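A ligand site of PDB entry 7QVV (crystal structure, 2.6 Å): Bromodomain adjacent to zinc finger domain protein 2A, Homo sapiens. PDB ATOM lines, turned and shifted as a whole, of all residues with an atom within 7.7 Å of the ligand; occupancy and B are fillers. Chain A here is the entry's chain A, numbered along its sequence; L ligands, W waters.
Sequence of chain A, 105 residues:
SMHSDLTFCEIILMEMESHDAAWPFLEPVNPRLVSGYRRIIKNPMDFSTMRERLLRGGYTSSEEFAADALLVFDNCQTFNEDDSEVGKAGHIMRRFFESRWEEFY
O of Val 86 sits at hydrogen-bond distance from SG of Cys 76, 3.6 Å away.
ND2 of Asn 80 sits at hydrogen-bond distance from O of Cys 76, at 3.1 Å.
Water W1 lies within hydrogen-bond range of an oxygen (O2) of the ligand (2.4 Å), the side-chain hydroxyl (OH) of Tyr 37 (2.5 Å), the backbone NH (N) of Cys 76 (3.4 Å) and the backbone carbonyl oxygen (O) of Asn 75 (3.5 Å).
O of Trp 23 touches C1 of the ligand (3.6 Å).
Pro 24 touches the ligand.
CG2 of Val 29 touches C9 of the ligand, 3.5 Å away.
CE1 of Tyr 37 touches O2 of the ligand, at 3.3 Å.
Phe 79 touches the ligand (CD2 to N3, 3.8 Å).
Val 86 touches the ligand (CG1 to C9, 3.5 Å).
Hydrophobic or aromatic side chains that line the ligand: Pro 24, Val 29, Tyr 37, Phe 79 and Val 86.
Eight residues have an atom within 4 Å of the ligand: Trp 23, Pro 24, Glu 27, Val 29, Tyr 37, Phe 79, Asn 80 and Val 86.
ND2 of Asn 80 sits at hydrogen-bond distance from O2 of the ligand, at 2.8 Å.
OE1 of Glu 27 lies within salt-bridge range of N1 of the ligand (2.6 Å).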
ATOM      1  N   ALA A  22     -27.987  14.859  15.345  1.00  0.00           N
ATOM      2  CA  ALA A  22     -27.974  15.119  16.770  1.00  0.00           C
ATOM      3  C   ALA A  22     -28.811  14.117  17.554  1.00  0.00           C
ATOM      4  O   ALA A  22     -28.630  13.994  18.771  1.00  0.00           O
ATOM      5  CB  ALA A  22     -28.503  16.527  17.057  1.00  0.00           C
ATOM      6  N   TRP A  23     -29.681  13.374  16.878  1.00  0.00           N
ATOM      7  CA  TRP A  23     -30.704  12.570  17.518  1.00  0.00           C
ATOM      8  C   TRP A  23     -30.224  11.625  18.619  1.00  0.00           C
ATOM      9  O   TRP A  23     -30.998  11.350  19.545  1.00  0.00           O
ATOM     10  CB  TRP A  23     -31.468  11.771  16.450  1.00  0.00           C
ATOM     11  CG  TRP A  23     -30.620  10.871  15.638  1.00  0.00           C
ATOM     12  CD1 TRP A  23     -29.978  11.170  14.482  1.00  0.00           C
ATOM     13  CD2 TRP A  23     -30.322   9.504  15.926  1.00  0.00           C
ATOM     14  NE1 TRP A  23     -29.292  10.074  14.026  1.00  0.00           N
ATOM     15  CE2 TRP A  23     -29.475   9.045  14.904  1.00  0.00           C
ATOM     16  CE3 TRP A  23     -30.665   8.635  16.962  1.00  0.00           C
ATOM     17  CZ2 TRP A  23     -28.986   7.746  14.864  1.00  0.00           C
ATOM     18  CZ3 TRP A  23     -30.177   7.340  16.935  1.00  0.00           C
ATOM     19  CH2 TRP A  23     -29.347   6.905  15.889  1.00  0.00           C
ATOM     20  N   PRO A  24     -28.996  11.083  18.598  1.00  0.00           N
ATOM     21  CA  PRO A  24     -28.613  10.216  19.730  1.00  0.00           C
ATOM     22  C   PRO A  24     -28.205  10.987  20.958  1.00  0.00           C
ATOM     23  O   PRO A  24     -27.987  10.381  22.015  1.00  0.00           O
ATOM     24  CB  PRO A  24     -27.382   9.469  19.202  1.00  0.00           C
ATOM     25  CG  PRO A  24     -27.400   9.623  17.723  1.00  0.00           C
ATOM     26  CD  PRO A  24     -28.007  10.983  17.510  1.00  0.00           C
ATOM     27  N   PHE A  25     -28.119  12.311  20.873  1.00  0.00           N
ATOM     28  CA  PHE A  25     -27.451  13.113  21.875  1.00  0.00           C
ATOM     29  C   PHE A  25     -28.356  14.200  22.427  1.00  0.00           C
ATOM     30  O   PHE A  25     -27.896  14.991  23.251  1.00  0.00           O
ATOM     31  CB  PHE A  25     -26.139  13.702  21.325  1.00  0.00           C
ATOM     32  CG  PHE A  25     -25.306  12.679  20.594  1.00  0.00           C
ATOM     33  CD1 PHE A  25     -24.732  11.631  21.288  1.00  0.00           C
ATOM     34  CD2 PHE A  25     -25.147  12.751  19.217  1.00  0.00           C
ATOM     35  CE1 PHE A  25     -23.980  10.675  20.629  1.00  0.00           C
ATOM     36  CE2 PHE A  25     -24.394  11.795  18.558  1.00  0.00           C
ATOM     37  CZ  PHE A  25     -23.812  10.750  19.266  1.00  0.00           C
ATOM     38  N   LEU A  26     -29.616  14.255  21.981  1.00  0.00           N
ATOM     39  CA  LEU A  26     -30.517  15.307  22.447  1.00  0.00           C
ATOM     40  C   LEU A  26     -30.933  15.104  23.896  1.00  0.00           C
ATOM     41  O   LEU A  26     -31.087  16.073  24.641  1.00  0.00           O
ATOM     42  CB  LEU A  26     -31.750  15.391  21.542  1.00  0.00           C
ATOM     43  CG  LEU A  26     -31.508  15.657  20.050  1.00  0.00           C
ATOM     44  CD1 LEU A  26     -32.814  15.576  19.289  1.00  0.00           C
ATOM     45  CD2 LEU A  26     -30.901  17.026  19.890  1.00  0.00           C
ATOM     46  N   GLU A  27     -31.138  13.856  24.314  1.00  0.00           N
ATOM     47  CA  GLU A  27     -31.505  13.553  25.693  1.00  0.00           C
ATOM     48  C   GLU A  27     -30.561  12.508  26.271  1.00  0.00           C
ATOM     49  O   GLU A  27     -30.003  11.694  25.529  1.00  0.00           O
ATOM     50  CB  GLU A  27     -32.958  13.037  25.776  1.00  0.00           C
ATOM     51  CG  GLU A  27     -33.397  12.174  24.597  1.00  0.00           C
ATOM     52  CD  GLU A  27     -34.530  11.237  24.961  1.00  0.00           C
ATOM     53  OE1 GLU A  27     -34.434  10.028  24.627  1.00  0.00           O
ATOM     54  OE2 GLU A  27     -35.498  11.693  25.592  1.00  0.00           O
ATOM     55  N   PRO A  28     -30.347  12.523  27.589  1.00  0.00           N
ATOM     56  CA  PRO A  28     -29.452  11.544  28.219  1.00  0.00           C
ATOM     57  C   PRO A  28     -29.788  10.122  27.803  1.00  0.00           C
ATOM     58  O   PRO A  28     -30.962   9.767  27.673  1.00  0.00           O
ATOM     59  CB  PRO A  28     -29.688  11.761  29.717  1.00  0.00           C
ATOM     60  CG  PRO A  28     -30.135  13.177  29.836  1.00  0.00           C
ATOM     61  CD  PRO A  28     -30.948  13.431  28.604  1.00  0.00           C
ATOM     62  N   VAL A  29     -28.768   9.300  27.598  1.00  0.00           N
ATOM     63  CA  VAL A  29     -29.033   7.896  27.313  1.00  0.00           C
ATOM     64  C   VAL A  29     -29.714   7.279  28.535  1.00  0.00           C
ATOM     65  O   VAL A  29     -29.263   7.461  29.672  1.00  0.00           O
ATOM     66  CB  VAL A  29     -27.717   7.168  26.998  1.00  0.00           C
ATOM     67  CG1 VAL A  29     -27.924   5.660  26.926  1.00  0.00           C
ATOM     68  CG2 VAL A  29     -27.128   7.690  25.705  1.00  0.00           C
ATOM     69  N   ASN A  30     -30.787   6.530  28.288  1.00  0.00           N
ATOM     70  CA  ASN A  30     -31.521   5.858  29.360  1.00  0.00           C
ATOM     71  C   ASN A  30     -30.959   4.452  29.579  1.00  0.00           C
ATOM     72  O   ASN A  30     -31.249   3.544  28.791  1.00  0.00           O
ATOM     73  CB  ASN A  30     -33.022   5.813  29.074  1.00  0.00           C
ATOM     74  CG  ASN A  30     -33.848   5.365  30.266  1.00  0.00           C
ATOM     75  OD1 ASN A  30     -33.328   4.851  31.259  1.00  0.00           O
ATOM     76  ND2 ASN A  30     -35.152   5.610  30.189  1.00  0.00           N
ATOM     77  N   LEU A  33     -32.832   1.141  28.998  1.00  0.00           N
ATOM     78  CA  LEU A  33     -33.106   0.697  27.639  1.00  0.00           C
ATOM     79  C   LEU A  33     -31.854   0.281  26.891  1.00  0.00           C
ATOM     80  O   LEU A  33     -31.945  -0.456  25.899  1.00  0.00           O
ATOM     81  CB  LEU A  33     -33.838   1.773  26.817  1.00  0.00           C
ATOM     82  CG  LEU A  33     -35.237   2.286  27.201  1.00  0.00           C
ATOM     83  CD1 LEU A  33     -36.184   1.136  27.292  1.00  0.00           C
ATOM     84  CD2 LEU A  33     -35.265   3.055  28.482  1.00  0.00           C
ATOM     85  N   VAL A  34     -30.690   0.699  27.349  1.00  0.00           N
ATOM     86  CA  VAL A  34     -29.434   0.407  26.667  1.00  0.00           C
ATOM     87  C   VAL A  34     -28.582  -0.482  27.556  1.00  0.00           C
ATOM     88  O   VAL A  34     -27.966  -0.020  28.519  1.00  0.00           O
ATOM     89  CB  VAL A  34     -28.697   1.692  26.294  1.00  0.00           C
ATOM     90  CG1 VAL A  34     -27.484   1.375  25.492  1.00  0.00           C
ATOM     91  CG2 VAL A  34     -29.614   2.641  25.532  1.00  0.00           C
ATOM     92  N   TYR A  37     -24.822   0.091  29.212  1.00  0.00           N
ATOM     93  CA  TYR A  37     -24.380   1.478  29.133  1.00  0.00           C
ATOM     94  C   TYR A  37     -23.872   1.973  30.488  1.00  0.00           C
ATOM     95  O   TYR A  37     -22.816   2.611  30.583  1.00  0.00           O
ATOM     96  CB  TYR A  37     -25.503   2.381  28.641  1.00  0.00           C
ATOM     97  CG  TYR A  37     -25.013   3.727  28.147  1.00  0.00           C
ATOM     98  CD1 TYR A  37     -24.486   3.863  26.881  1.00  0.00           C
ATOM     99  CD2 TYR A  37     -25.061   4.847  28.963  1.00  0.00           C
ATOM    100  CE1 TYR A  37     -24.039   5.086  26.431  1.00  0.00           C
ATOM    101  CE2 TYR A  37     -24.603   6.087  28.523  1.00  0.00           C
ATOM    102  CZ  TYR A  37     -24.088   6.192  27.250  1.00  0.00           C
ATOM    103  OH  TYR A  37     -23.629   7.424  26.783  1.00  0.00           O
ATOM    104  N   ILE A  41     -20.175   3.286  30.379  1.00  0.00           N
ATOM    105  CA  ILE A  41     -19.992   4.733  30.313  1.00  0.00           C
ATOM    106  C   ILE A  41     -20.026   5.292  31.732  1.00  0.00           C
ATOM    107  O   ILE A  41     -21.080   5.302  32.378  1.00  0.00           O
ATOM    108  CB  ILE A  41     -21.063   5.404  29.443  1.00  0.00           C
ATOM    109  CG1 ILE A  41     -20.881   5.024  27.977  1.00  0.00           C
ATOM    110  CG2 ILE A  41     -21.004   6.907  29.620  1.00  0.00           C
ATOM    111  CD1 ILE A  41     -19.516   5.353  27.398  1.00  0.00           C
ATOM    112  N   MET A  45     -23.124  12.085  29.129  1.00  0.00           N
ATOM    113  CA  MET A  45     -23.266  13.491  28.799  1.00  0.00           C
ATOM    114  C   MET A  45     -24.091  13.550  27.530  1.00  0.00           C
ATOM    115  O   MET A  45     -24.068  12.638  26.709  1.00  0.00           O
ATOM    116  CB  MET A  45     -21.903  14.177  28.614  1.00  0.00           C
ATOM    117  CG  MET A  45     -22.004  15.689  28.380  1.00  0.00           C
ATOM    118  SD  MET A  45     -22.965  16.595  29.636  1.00  0.00           S
ATOM    119  CE  MET A  45     -21.982  16.289  31.100  1.00  0.00           C
ATOM    120  N   VAL A  72     -19.439  13.773  25.258  1.00  0.00           N
ATOM    121  CA  VAL A  72     -20.552  13.193  24.505  1.00  0.00           C
ATOM    122  C   VAL A  72     -20.023  12.229  23.452  1.00  0.00           C
ATOM    123  O   VAL A  72     -20.471  11.085  23.329  1.00  0.00           O
ATOM    124  CB  VAL A  72     -21.407  14.300  23.868  1.00  0.00           C
ATOM    125  CG1 VAL A  72     -22.451  13.688  22.958  1.00  0.00           C
ATOM    126  CG2 VAL A  72     -22.048  15.129  24.927  1.00  0.00           C
ATOM    127  N   ASN A  75     -17.884   9.146  24.839  1.00  0.00           N
ATOM    128  CA  ASN A  75     -18.872   8.161  25.240  1.00  0.00           C
ATOM    129  C   ASN A  75     -19.440   7.429  24.036  1.00  0.00           C
ATOM    130  O   ASN A  75     -19.491   6.195  24.014  1.00  0.00           O
ATOM    131  CB  ASN A  75     -19.985   8.853  26.013  1.00  0.00           C
ATOM    132  CG  ASN A  75     -19.529   9.316  27.369  1.00  0.00           C
ATOM    133  OD1 ASN A  75     -18.517   8.838  27.880  1.00  0.00           O
ATOM    134  ND2 ASN A  75     -20.265  10.260  27.943  1.00  0.00           N
ATOM    135  N   CYS A  76     -19.799   8.170  22.989  1.00  0.00           N
ATOM    136  CA  CYS A  76     -20.423   7.548  21.837  1.00  0.00           C
ATOM    137  C   CYS A  76     -19.509   6.498  21.215  1.00  0.00           C
ATOM    138  O   CYS A  76     -19.927   5.361  20.951  1.00  0.00           O
ATOM    139  CB  CYS A  76     -20.788   8.613  20.801  1.00  0.00           C
ATOM    140  SG  CYS A  76     -21.667   7.953  19.395  1.00  0.00           S
ATOM    141  N   GLN A  77     -18.232   6.850  21.025  1.00  0.00           N
ATOM    142  CA  GLN A  77     -17.257   5.962  20.416  1.00  0.00           C
ATOM    143  C   GLN A  77     -16.879   4.815  21.330  1.00  0.00           C
ATOM    144  O   GLN A  77     -16.552   3.732  20.851  1.00  0.00           O
ATOM    145  CB  GLN A  77     -16.022   6.775  20.044  1.00  0.00           C
ATOM    146  CG  GLN A  77     -16.266   7.766  18.925  1.00  0.00           C
ATOM    147  CD  GLN A  77     -15.066   8.646  18.687  1.00  0.00           C
ATOM    148  OE1 GLN A  77     -14.196   8.335  17.895  1.00  0.00           O
ATOM    149  NE2 GLN A  77     -14.999   9.755  19.430  1.00  0.00           N
ATOM    150  N   THR A  78     -16.943   5.016  22.657  1.00  0.00           N
ATOM    151  CA  THR A  78     -16.702   3.936  23.603  1.00  0.00           C
ATOM    152  C   THR A  78     -17.834   2.915  23.592  1.00  0.00           C
ATOM    153  O   THR A  78     -17.590   1.701  23.682  1.00  0.00           O
ATOM    154  CB  THR A  78     -16.586   4.498  25.028  1.00  0.00           C
ATOM    155  OG1 THR A  78     -15.509   5.426  25.132  1.00  0.00           O
ATOM    156  CG2 THR A  78     -16.351   3.385  26.013  1.00  0.00           C
ATOM    157  N   PHE A  79     -19.082   3.353  23.511  1.00  0.00           N
ATOM    158  CA  PHE A  79     -20.157   2.388  23.604  1.00  0.00           C
ATOM    159  C   PHE A  79     -20.623   1.813  22.268  1.00  0.00           C
ATOM    160  O   PHE A  79     -21.038   0.652  22.219  1.00  0.00           O
ATOM    161  CB  PHE A  79     -21.379   2.996  24.287  1.00  0.00           C
ATOM    162  CG  PHE A  79     -22.469   2.005  24.558  1.00  0.00           C
ATOM    163  CD1 PHE A  79     -22.364   1.142  25.637  1.00  0.00           C
ATOM    164  CD2 PHE A  79     -23.540   1.883  23.688  1.00  0.00           C
ATOM    165  CE1 PHE A  79     -23.346   0.224  25.891  1.00  0.00           C
ATOM    166  CE2 PHE A  79     -24.523   0.938  23.928  1.00  0.00           C
ATOM    167  CZ  PHE A  79     -24.417   0.106  25.035  1.00  0.00           C
ATOM    168  N   ASN A  80     -20.485   2.560  21.178  1.00  0.00           N
ATOM    169  CA  ASN A  80     -21.043   2.161  19.902  1.00  0.00           C
ATOM    170  C   ASN A  80     -19.971   1.887  18.879  1.00  0.00           C
ATOM    171  O   ASN A  80     -18.974   2.616  18.787  1.00  0.00           O
ATOM    172  CB  ASN A  80     -21.965   3.235  19.330  1.00  0.00           C
ATOM    173  CG  ASN A  80     -23.093   3.601  20.248  1.00  0.00           C
ATOM    174  OD1 ASN A  80     -24.122   2.921  20.293  1.00  0.00           O
ATOM    175  ND2 ASN A  80     -22.910   4.670  21.017  1.00  0.00           N
ATOM    176  N   SER A  84     -22.190   1.556  13.672  1.00  0.00           N
ATOM    177  CA  SER A  84     -23.543   1.595  14.197  1.00  0.00           C
ATOM    178  C   SER A  84     -24.201   2.910  13.817  1.00  0.00           C
ATOM    179  O   SER A  84     -23.535   3.917  13.585  1.00  0.00           O
ATOM    180  CB  SER A  84     -23.527   1.444  15.711  1.00  0.00           C
ATOM    181  OG  SER A  84     -23.078   2.652  16.289  1.00  0.00           O
ATOM    182  N   VAL A  86     -25.953   4.991  15.663  1.00  0.00           N
ATOM    183  CA  VAL A  86     -25.588   6.005  16.629  1.00  0.00           C
ATOM    184  C   VAL A  86     -24.128   6.388  16.453  1.00  0.00           C
ATOM    185  O   VAL A  86     -23.791   7.578  16.496  1.00  0.00           O
ATOM    186  CB  VAL A  86     -25.864   5.514  18.077  1.00  0.00           C
ATOM    187  CG1 VAL A  86     -25.285   6.488  19.103  1.00  0.00           C
ATOM    188  CG2 VAL A  86     -27.353   5.337  18.313  1.00  0.00           C
ATOM    189  N   GLY A  87     -23.243   5.409  16.275  1.00  0.00           N
ATOM    190  CA  GLY A  87     -21.827   5.711  16.062  1.00  0.00           C
ATOM    191  C   GLY A  87     -21.599   6.586  14.834  1.00  0.00           C
ATOM    192  O   GLY A  87     -20.798   7.522  14.876  1.00  0.00           O
HETATM  193  C1  LIG L   1     -32.582   8.875  21.567  1.00  0.00           C
HETATM  194  C2  LIG L   1     -32.838   7.606  20.774  1.00  0.00           C
HETATM  195  C3  LIG L   1     -31.881   6.399  21.018  1.00  0.00           C
HETATM  196  C4  LIG L   1     -30.273   8.118  21.942  1.00  0.00           C
HETATM  197  C5  LIG L   1     -31.536   8.711  22.612  1.00  0.00           C
HETATM  198  C6  LIG L   1     -29.379   5.556  21.541  1.00  0.00           C
HETATM  199  C7  LIG L   1     -27.942   5.735  22.005  1.00  0.00           C
HETATM  200  C8  LIG L   1     -27.299   6.962  22.023  1.00  0.00           C
HETATM  201  C9  LIG L   1     -25.960   7.009  22.464  1.00  0.00           C
HETATM  202  C10 LIG L   1     -25.325   5.808  22.844  1.00  0.00           C
HETATM  203  C11 LIG L   1     -27.243   4.574  22.392  1.00  0.00           C
HETATM  204  N1  LIG L   1     -33.856   9.316  22.246  1.00  0.00           N
HETATM  205  N2  LIG L   1     -30.460   6.663  21.514  1.00  0.00           N
HETATM  206  N3  LIG L   1     -25.973   4.636  22.809  1.00  0.00           N
HETATM  207  O1  LIG L   1     -29.694   4.468  21.179  1.00  0.00           O
HETATM  208  O2  LIG L   1     -24.223   5.848  23.208  1.00  0.00           O
HETATM  209  O   HOH W   1     -22.746   7.313  24.426  1.00  0.00           O
HETATM  210  O   HOH W   2     -32.595   4.737  23.923  1.00  0.00           O
HETATM  211  O   HOH W   3     -32.278   6.931  25.508  1.00  0.00           O
